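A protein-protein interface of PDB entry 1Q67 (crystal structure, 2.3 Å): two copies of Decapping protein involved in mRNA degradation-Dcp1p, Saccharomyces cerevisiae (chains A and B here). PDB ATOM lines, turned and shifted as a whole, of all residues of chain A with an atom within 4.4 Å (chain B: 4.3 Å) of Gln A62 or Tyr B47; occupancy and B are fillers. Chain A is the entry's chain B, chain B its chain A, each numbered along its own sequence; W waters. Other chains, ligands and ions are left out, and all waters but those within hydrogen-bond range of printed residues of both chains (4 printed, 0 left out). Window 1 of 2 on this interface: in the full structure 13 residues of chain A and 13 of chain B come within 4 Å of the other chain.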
ATOM      1  N   ALA A  44       8.896  -3.908   6.743  1.00  0.00           N
ATOM      2  CA  ALA A  44       9.971  -3.953   5.759  1.00  0.00           C
ATOM      3  C   ALA A  44      11.218  -4.475   6.450  1.00  0.00           C
ATOM      4  O   ALA A  44      11.506  -4.098   7.580  1.00  0.00           O
ATOM      5  CB  ALA A  44      10.226  -2.565   5.191  1.00  0.00           C
ATOM      6  N   SER A  45      11.953  -5.343   5.770  1.00  0.00           N
ATOM      7  CA  SER A  45      13.162  -5.920   6.342  1.00  0.00           C
ATOM      8  C   SER A  45      14.354  -5.542   5.456  1.00  0.00           C
ATOM      9  O   SER A  45      14.278  -5.627   4.229  1.00  0.00           O
ATOM     10  CB  SER A  45      13.009  -7.443   6.442  1.00  0.00           C
ATOM     11  OG  SER A  45      14.101  -8.008   7.141  1.00  0.00           O
ATOM     12  N   LYS A  58      21.695 -10.272   5.833  1.00  0.00           N
ATOM     13  CA  LYS A  58      20.580  -9.713   6.584  1.00  0.00           C
ATOM     14  C   LYS A  58      21.110  -8.708   7.595  1.00  0.00           C
ATOM     15  O   LYS A  58      22.044  -9.007   8.342  1.00  0.00           O
ATOM     16  CB  LYS A  58      19.826 -10.837   7.307  1.00  0.00           C
ATOM     17  CG  LYS A  58      18.782 -10.367   8.312  1.00  0.00           C
ATOM     18  CD  LYS A  58      17.752  -9.432   7.687  1.00  0.00           C
ATOM     19  CE  LYS A  58      16.851  -8.850   8.774  1.00  0.00           C
ATOM     20  NZ  LYS A  58      16.197  -7.566   8.405  1.00  0.00           N
ATOM     21  N   LEU A  59      20.542  -7.507   7.607  1.00  0.00           N
ATOM     22  CA  LEU A  59      20.965  -6.497   8.570  1.00  0.00           C
ATOM     23  C   LEU A  59      19.941  -6.450   9.702  1.00  0.00           C
ATOM     24  O   LEU A  59      18.799  -6.879   9.528  1.00  0.00           O
ATOM     25  CB  LEU A  59      21.074  -5.117   7.913  1.00  0.00           C
ATOM     26  CG  LEU A  59      22.083  -4.960   6.772  1.00  0.00           C
ATOM     27  CD1 LEU A  59      22.174  -3.489   6.392  1.00  0.00           C
ATOM     28  CD2 LEU A  59      23.453  -5.487   7.207  1.00  0.00           C
ATOM     29  N   GLU A  60      20.342  -5.911  10.848  1.00  0.00           N
ATOM     30  CA  GLU A  60      19.463  -5.847  12.014  1.00  0.00           C
ATOM     31  C   GLU A  60      18.373  -4.779  11.981  1.00  0.00           C
ATOM     32  O   GLU A  60      18.155  -4.088  12.971  1.00  0.00           O
ATOM     33  CB  GLU A  60      20.297  -5.664  13.291  1.00  0.00           C
ATOM     34  CG  GLU A  60      21.314  -6.770  13.537  1.00  0.00           C
ATOM     35  CD  GLU A  60      21.803  -6.820  14.984  1.00  0.00           C
ATOM     36  OE1 GLU A  60      22.220  -5.763  15.523  1.00  0.00           O
ATOM     37  OE2 GLU A  60      21.771  -7.925  15.580  1.00  0.00           O
ATOM     38  N   TYR A  61      17.689  -4.630  10.856  1.00  0.00           N
ATOM     39  CA  TYR A  61      16.629  -3.633  10.778  1.00  0.00           C
ATOM     40  C   TYR A  61      15.405  -4.172  10.067  1.00  0.00           C
ATOM     41  O   TYR A  61      15.506  -4.705   8.957  1.00  0.00           O
ATOM     42  CB  TYR A  61      17.113  -2.369  10.060  1.00  0.00           C
ATOM     43  CG  TYR A  61      18.313  -1.717  10.705  1.00  0.00           C
ATOM     44  CD1 TYR A  61      19.599  -1.983  10.243  1.00  0.00           C
ATOM     45  CD2 TYR A  61      18.165  -0.851  11.792  1.00  0.00           C
ATOM     46  CE1 TYR A  61      20.716  -1.409  10.840  1.00  0.00           C
ATOM     47  CE2 TYR A  61      19.276  -0.266  12.406  1.00  0.00           C
ATOM     48  CZ  TYR A  61      20.550  -0.555  11.920  1.00  0.00           C
ATOM     49  OH  TYR A  61      21.663  -0.004  12.502  1.00  0.00           O
ATOM     50  N   GLN A  62      14.259  -4.046  10.732  1.00  0.00           N
ATOM     51  CA  GLN A  62      12.960  -4.489  10.207  1.00  0.00           C
ATOM     52  C   GLN A  62      11.923  -3.683  10.971  1.00  0.00           C
ATOM     53  O   GLN A  62      12.054  -3.492  12.179  1.00  0.00           O
ATOM     54  CB  GLN A  62      12.663  -5.962  10.515  1.00  0.00           C
ATOM     55  CG  GLN A  62      13.823  -6.912  10.452  1.00  0.00           C
ATOM     56  CD  GLN A  62      14.875  -6.614  11.488  1.00  0.00           C
ATOM     57  OE1 GLN A  62      14.571  -6.182  12.602  1.00  0.00           O
ATOM     58  NE2 GLN A  62      16.121  -6.851  11.133  1.00  0.00           N
ATOM     59  N   GLY A  63      10.882  -3.246  10.282  1.00  0.00           N
ATOM     60  CA  GLY A  63       9.854  -2.467  10.940  1.00  0.00           C
ATOM     61  C   GLY A  63       9.175  -1.516   9.981  1.00  0.00           C
ATOM     62  O   GLY A  63       9.047  -1.810   8.795  1.00  0.00           O
ATOM     63  N   ILE A 144      13.827   3.301   8.467  1.00  0.00           N
ATOM     64  CA  ILE A 144      13.180   2.081   8.902  1.00  0.00           C
ATOM     65  C   ILE A 144      13.261   2.117  10.427  1.00  0.00           C
ATOM     66  O   ILE A 144      14.351   2.227  11.001  1.00  0.00           O
ATOM     67  CB  ILE A 144      13.885   0.828   8.379  1.00  0.00           C
ATOM     68  CG1 ILE A 144      13.729   0.740   6.855  1.00  0.00           C
ATOM     69  CG2 ILE A 144      13.269  -0.407   9.027  1.00  0.00           C
ATOM     70  CD1 ILE A 144      14.515  -0.386   6.232  1.00  0.00           C
ATOM     71  N   LEU A 145      12.102   2.051  11.074  1.00  0.00           N
ATOM     72  CA  LEU A 145      12.040   2.100  12.530  1.00  0.00           C
ATOM     73  C   LEU A 145      11.730   0.716  13.073  1.00  0.00           C
ATOM     74  O   LEU A 145      10.621   0.222  12.888  1.00  0.00           O
ATOM     75  CB  LEU A 145      10.941   3.074  12.967  1.00  0.00           C
ATOM     76  CG  LEU A 145      11.018   4.512  12.433  1.00  0.00           C
ATOM     77  CD1 LEU A 145       9.627   5.091  12.278  1.00  0.00           C
ATOM     78  CD2 LEU A 145      11.846   5.360  13.365  1.00  0.00           C
ATOM     79  N   ASN A 146      12.699   0.082  13.729  1.00  0.00           N
ATOM     80  CA  ASN A 146      12.460  -1.252  14.290  1.00  0.00           C
ATOM     81  C   ASN A 146      11.289  -1.242  15.261  1.00  0.00           C
ATOM     82  O   ASN A 146      11.158  -0.329  16.074  1.00  0.00           O
ATOM     83  CB  ASN A 146      13.709  -1.783  14.999  1.00  0.00           C
ATOM     84  CG  ASN A 146      14.758  -2.268  14.021  1.00  0.00           C
ATOM     85  OD1 ASN A 146      14.544  -2.232  12.807  1.00  0.00           O
ATOM     86  ND2 ASN A 146      15.894  -2.729  14.538  1.00  0.00           N
ATOM     87  N   ARG A 147      10.440  -2.261  15.153  1.00  0.00           N
ATOM     88  CA  ARG A 147       9.254  -2.406  15.995  1.00  0.00           C
ATOM     89  C   ARG A 147       9.539  -3.169  17.278  1.00  0.00           C
ATOM     90  O   ARG A 147       8.960  -2.881  18.323  1.00  0.00           O
ATOM     91  CB  ARG A 147       8.161  -3.169  15.245  1.00  0.00           C
ATOM     92  CG  ARG A 147       7.396  -2.393  14.191  1.00  0.00           C
ATOM     93  CD  ARG A 147       6.568  -3.363  13.354  1.00  0.00           C
ATOM     94  NE  ARG A 147       5.623  -2.683  12.477  1.00  0.00           N
ATOM     95  CZ  ARG A 147       4.489  -2.133  12.894  1.00  0.00           C
ATOM     96  NH1 ARG A 147       4.164  -2.195  14.180  1.00  0.00           N
ATOM     97  NH2 ARG A 147       3.690  -1.514  12.032  1.00  0.00           N
ATOM     98  N   ILE A 148      10.422  -4.154  17.183  1.00  0.00           N
ATOM     99  CA  ILE A 148      10.755  -5.006  18.318  1.00  0.00           C
ATOM    100  C   ILE A 148      11.841  -4.446  19.234  1.00  0.00           C
ATOM    101  O   ILE A 148      11.967  -4.879  20.379  1.00  0.00           O
ATOM    102  CB  ILE A 148      11.146  -6.415  17.821  1.00  0.00           C
ATOM    103  CG1 ILE A 148      10.116  -6.892  16.790  1.00  0.00           C
ATOM    104  CG2 ILE A 148      11.185  -7.395  18.986  1.00  0.00           C
ATOM    105  CD1 ILE A 148       8.665  -6.848  17.276  1.00  0.00           C
ATOM    106  N   SER B  45       9.947 -13.857  11.532  1.00  0.00           N
ATOM    107  CA  SER B  45      11.252 -13.295  11.837  1.00  0.00           C
ATOM    108  C   SER B  45      11.703 -13.676  13.256  1.00  0.00           C
ATOM    109  O   SER B  45      10.944 -13.543  14.223  1.00  0.00           O
ATOM    110  CB  SER B  45      11.186 -11.776  11.674  1.00  0.00           C
ATOM    111  OG  SER B  45      12.458 -11.199  11.872  1.00  0.00           O
ATOM    112  N   LEU B  46      12.950 -14.121  13.380  1.00  0.00           N
ATOM    113  CA  LEU B  46      13.474 -14.569  14.663  1.00  0.00           C
ATOM    114  C   LEU B  46      14.301 -13.587  15.474  1.00  0.00           C
ATOM    115  O   LEU B  46      15.168 -12.880  14.948  1.00  0.00           O
ATOM    116  CB  LEU B  46      14.293 -15.842  14.478  1.00  0.00           C
ATOM    117  CG  LEU B  46      14.698 -16.535  15.778  1.00  0.00           C
ATOM    118  CD1 LEU B  46      13.444 -17.150  16.439  1.00  0.00           C
ATOM    119  CD2 LEU B  46      15.728 -17.618  15.483  1.00  0.00           C
ATOM    120  N   TYR B  47      14.026 -13.582  16.776  1.00  0.00           N
ATOM    121  CA  TYR B  47      14.717 -12.737  17.732  1.00  0.00           C
ATOM    122  C   TYR B  47      15.152 -13.588  18.918  1.00  0.00           C
ATOM    123  O   TYR B  47      14.629 -14.684  19.144  1.00  0.00           O
ATOM    124  CB  TYR B  47      13.797 -11.630  18.255  1.00  0.00           C
ATOM    125  CG  TYR B  47      13.375 -10.605  17.229  1.00  0.00           C
ATOM    126  CD1 TYR B  47      12.320 -10.852  16.355  1.00  0.00           C
ATOM    127  CD2 TYR B  47      14.039  -9.377  17.136  1.00  0.00           C
ATOM    128  CE1 TYR B  47      11.930  -9.894  15.406  1.00  0.00           C
ATOM    129  CE2 TYR B  47      13.662  -8.419  16.198  1.00  0.00           C
ATOM    130  CZ  TYR B  47      12.611  -8.681  15.337  1.00  0.00           C
ATOM    131  OH  TYR B  47      12.251  -7.734  14.410  1.00  0.00           O
ATOM    132  N   LYS B  48      16.112 -13.081  19.676  1.00  0.00           N
ATOM    133  CA  LYS B  48      16.560 -13.789  20.860  1.00  0.00           C
ATOM    134  C   LYS B  48      16.636 -12.794  22.007  1.00  0.00           C
ATOM    135  O   LYS B  48      17.117 -11.671  21.840  1.00  0.00           O
ATOM    136  CB  LYS B  48      17.918 -14.450  20.642  1.00  0.00           C
ATOM    137  CG  LYS B  48      18.286 -15.383  21.784  1.00  0.00           C
ATOM    138  CD  LYS B  48      19.556 -16.168  21.510  1.00  0.00           C
ATOM    139  CE  LYS B  48      19.796 -17.187  22.608  1.00  0.00           C
ATOM    140  NZ  LYS B  48      21.027 -17.987  22.368  1.00  0.00           N
ATOM    141  N   TRP B  56      15.488  -7.444  23.114  1.00  0.00           N
ATOM    142  CA  TRP B  56      15.426  -8.434  22.045  1.00  0.00           C
ATOM    143  C   TRP B  56      16.492  -8.186  20.980  1.00  0.00           C
ATOM    144  O   TRP B  56      16.554  -7.100  20.412  1.00  0.00           O
ATOM    145  CB  TRP B  56      14.068  -8.383  21.352  1.00  0.00           C
ATOM    146  CG  TRP B  56      12.938  -8.963  22.120  1.00  0.00           C
ATOM    147  CD1 TRP B  56      11.875  -8.291  22.644  1.00  0.00           C
ATOM    148  CD2 TRP B  56      12.711 -10.350  22.383  1.00  0.00           C
ATOM    149  NE1 TRP B  56      10.993  -9.173  23.210  1.00  0.00           N
ATOM    150  CE2 TRP B  56      11.478 -10.445  23.066  1.00  0.00           C
ATOM    151  CE3 TRP B  56      13.428 -11.523  22.106  1.00  0.00           C
ATOM    152  CZ2 TRP B  56      10.940 -11.673  23.478  1.00  0.00           C
ATOM    153  CZ3 TRP B  56      12.894 -12.747  22.517  1.00  0.00           C
ATOM    154  CH2 TRP B  56      11.660 -12.808  23.196  1.00  0.00           C
ATOM    155  N   ASN B  57      17.321  -9.191  20.709  1.00  0.00           N
ATOM    156  CA  ASN B  57      18.340  -9.073  19.668  1.00  0.00           C
ATOM    157  C   ASN B  57      17.785  -9.715  18.397  1.00  0.00           C
ATOM    158  O   ASN B  57      17.288 -10.843  18.432  1.00  0.00           O
ATOM    159  CB  ASN B  57      19.635  -9.805  20.048  1.00  0.00           C
ATOM    160  CG  ASN B  57      20.360  -9.165  21.224  1.00  0.00           C
ATOM    161  OD1 ASN B  57      20.549  -7.946  21.276  1.00  0.00           O
ATOM    162  ND2 ASN B  57      20.789  -9.995  22.168  1.00  0.00           N
ATOM    163  N   LYS B  58      17.863  -9.004  17.277  1.00  0.00           N
ATOM    164  CA  LYS B  58      17.385  -9.562  16.020  1.00  0.00           C
ATOM    165  C   LYS B  58      18.400 -10.586  15.519  1.00  0.00           C
ATOM    166  O   LYS B  58      19.586 -10.295  15.443  1.00  0.00           O
ATOM    167  CB  LYS B  58      17.208  -8.448  14.977  1.00  0.00           C
ATOM    168  CG  LYS B  58      16.994  -8.939  13.549  1.00  0.00           C
ATOM    169  CD  LYS B  58      15.820  -9.913  13.447  1.00  0.00           C
ATOM    170  CE  LYS B  58      15.721 -10.507  12.041  1.00  0.00           C
ATOM    171  NZ  LYS B  58      14.994 -11.808  12.001  1.00  0.00           N
ATOM    172  N   LEU B  59      17.946 -11.790  15.194  1.00  0.00           N
ATOM    173  CA  LEU B  59      18.862 -12.808  14.676  1.00  0.00           C
ATOM    174  C   LEU B  59      18.760 -12.849  13.147  1.00  0.00           C
ATOM    175  O   LEU B  59      17.783 -12.369  12.570  1.00  0.00           O
ATOM    176  CB  LEU B  59      18.553 -14.192  15.268  1.00  0.00           C
ATOM    177  CG  LEU B  59      18.737 -14.394  16.784  1.00  0.00           C
ATOM    178  CD1 LEU B  59      18.570 -15.879  17.110  1.00  0.00           C
ATOM    179  CD2 LEU B  59      20.126 -13.931  17.229  1.00  0.00           C
ATOM    180  N   TYR B 201      13.481 -17.365  22.843  1.00  0.00           N
ATOM    181  CA  TYR B 201      13.421 -16.841  21.490  1.00  0.00           C
ATOM    182  C   TYR B 201      12.076 -16.170  21.247  1.00  0.00           C
ATOM    183  O   TYR B 201      11.065 -16.518  21.873  1.00  0.00           O
ATOM    184  CB  TYR B 201      13.619 -17.959  20.458  1.00  0.00           C
ATOM    185  CG  TYR B 201      14.991 -18.592  20.475  1.00  0.00           C
ATOM    186  CD1 TYR B 201      15.268 -19.688  21.293  1.00  0.00           C
ATOM    187  CD2 TYR B 201      16.022 -18.084  19.684  1.00  0.00           C
ATOM    188  CE1 TYR B 201      16.545 -20.266  21.319  1.00  0.00           C
ATOM    189  CE2 TYR B 201      17.293 -18.644  19.703  1.00  0.00           C
ATOM    190  CZ  TYR B 201      17.553 -19.735  20.519  1.00  0.00           C
ATOM    191  OH  TYR B 201      18.816 -20.289  20.532  1.00  0.00           O
ATOM    192  N   GLY B 202      12.079 -15.203  20.336  1.00  0.00           N
ATOM    193  CA  GLY B 202      10.863 -14.492  19.985  1.00  0.00           C
ATOM    194  C   GLY B 202      10.648 -14.593  18.483  1.00  0.00           C
ATOM    195  O   GLY B 202      11.574 -14.376  17.698  1.00  0.00           O
ATOM    196  N   TRP B 204       8.346 -13.255  15.253  1.00  0.00           N
ATOM    197  CA  TRP B 204       7.344 -12.337  14.741  1.00  0.00           C
ATOM    198  C   TRP B 204       6.724 -12.953  13.502  1.00  0.00           C
ATOM    199  O   TRP B 204       7.426 -13.379  12.583  1.00  0.00           O
ATOM    200  CB  TRP B 204       7.947 -10.981  14.374  1.00  0.00           C
ATOM    201  CG  TRP B 204       6.870 -10.008  14.016  1.00  0.00           C
ATOM    202  CD1 TRP B 204       6.065  -9.333  14.883  1.00  0.00           C
ATOM    203  CD2 TRP B 204       6.390  -9.700  12.702  1.00  0.00           C
ATOM    204  NE1 TRP B 204       5.110  -8.629  14.195  1.00  0.00           N
ATOM    205  CE2 TRP B 204       5.285  -8.836  12.854  1.00  0.00           C
ATOM    206  CE3 TRP B 204       6.782 -10.076  11.412  1.00  0.00           C
ATOM    207  CZ2 TRP B 204       4.565  -8.338  11.763  1.00  0.00           C
ATOM    208  CZ3 TRP B 204       6.064  -9.577  10.321  1.00  0.00           C
ATOM    209  CH2 TRP B 204       4.968  -8.718  10.509  1.00  0.00           C
HETATM  210  O   HOH W   1      13.555  -4.966  22.332  1.00  0.00           O
HETATM  211  O   HOH W   2      12.072  -5.032  14.861  1.00  0.00           O
HETATM  212  O   HOH W   3      12.822  -9.633   9.247  1.00  0.00           O
HETATM  213  O   HOH W   4      19.211  -6.595  17.233  1.00  0.00           O
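OH of Tyr B47 lies within hydrogen-bond range of OE1 of Gln A62 (3.3 Å).
OE2 of Glu A60 lies close to O of Lys B58 (3.2 Å).
The backbone carbonyl oxygen (O) of Leu A59 sits at hydrogen-bond distance from the side-chain amide nitrogen (NE2) of Gln A62, at 3.1 Å.
The side-chain hydroxyl (OG) of Ser B45 sits at hydrogen-bond distance from the side-chain amino group (NZ) of Lys B58, at 2.6 Å.
The backbone NH (N) of Gln A62 is in hydrogen-bond range of the side-chain amide oxygen (OD1) of Asn A146 (2.8 Å).
OG of Ser A45 lies within hydrogen-bond range of NZ of Lys A58.
O of Gly B202 sits at hydrogen-bond distance from N of Tyr B47 (2.7 Å).
The backbone carbonyl oxygen of Glu A60 lies within hydrogen-bond range of the side-chain amide nitrogen of Asn A146 (3.1 Å).
Among the printed residues, pairs that only touch across the chains: Ile A148 with Tyr B47, Gln A62 with Lys B58, Ile A148 with Trp B56 and Lys A58 with Lys B58.
Of the printed residues of chain B, Gln A62 touches Tyr B47 (3.3 Å) and Lys B58 (3.3 Å).
Of chain A, only Gln A62 (3.3 Å) and Ile A148 (3.3 Å) come within 4 Å of Tyr B47.
Of the printed residues of chain A, Lys B58 touches Lys A58, Glu A60 and Gln A62.
Of the printed residues of chain B, Lys A58 touches Lys B58 (3.8 Å).
Of the printed residues of chain B, Ile A148 touches Tyr B47 (3.3 Å) and Trp B56 (3.8 Å).
Leu A145 touches none of the printed residues of chain B.
The nearest printed residue of chain A that does not touch Tyr B47 is Arg A147 (5.8 Å).
The nearest printed residue of chain B that does not touch Lys A58 is Leu B59 (4.8 Å).
Of the 13 printed residues of chain A, 4 touch a printed residue of chain B.
Of the 11 printed residues of chain B, 3 touch a printed residue of chain A.
Hydrophobic or aromatic side chains of chain B that line the printed part of chain A: Tyr B47 and Trp B56.
Among the printed residues, 6 pairs touch across the chains.
Lys B58 touches its own counterpart, Lys A58.
Positions printed for both chains: 45, 58 and 59.
Of the 6 pairs that touch across the chains among the printed residues, 1 has its exchanged pair printed and touching as well.
Water W1 lies within hydrogen-bond range of O of Ile A148 and N of Trp B56.
Water W2 lies within hydrogen-bond range of the side-chain hydroxyl of Tyr B47 (2.7 Å), the backbone NH of Ile A148 (3.0 Å), the backbone carbonyl oxygen of Gln A62 (3.1 Å) and the backbone NH of Arg A147 (3.2 Å).
Water W4 bridges the backbone NH (N) of Lys B58 (2.8 Å) and the side-chain carboxylate (OE2) of Glu A60 (3.3 Å).
Water W3 bridges OG of Ser A45 and OG of Ser B45.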
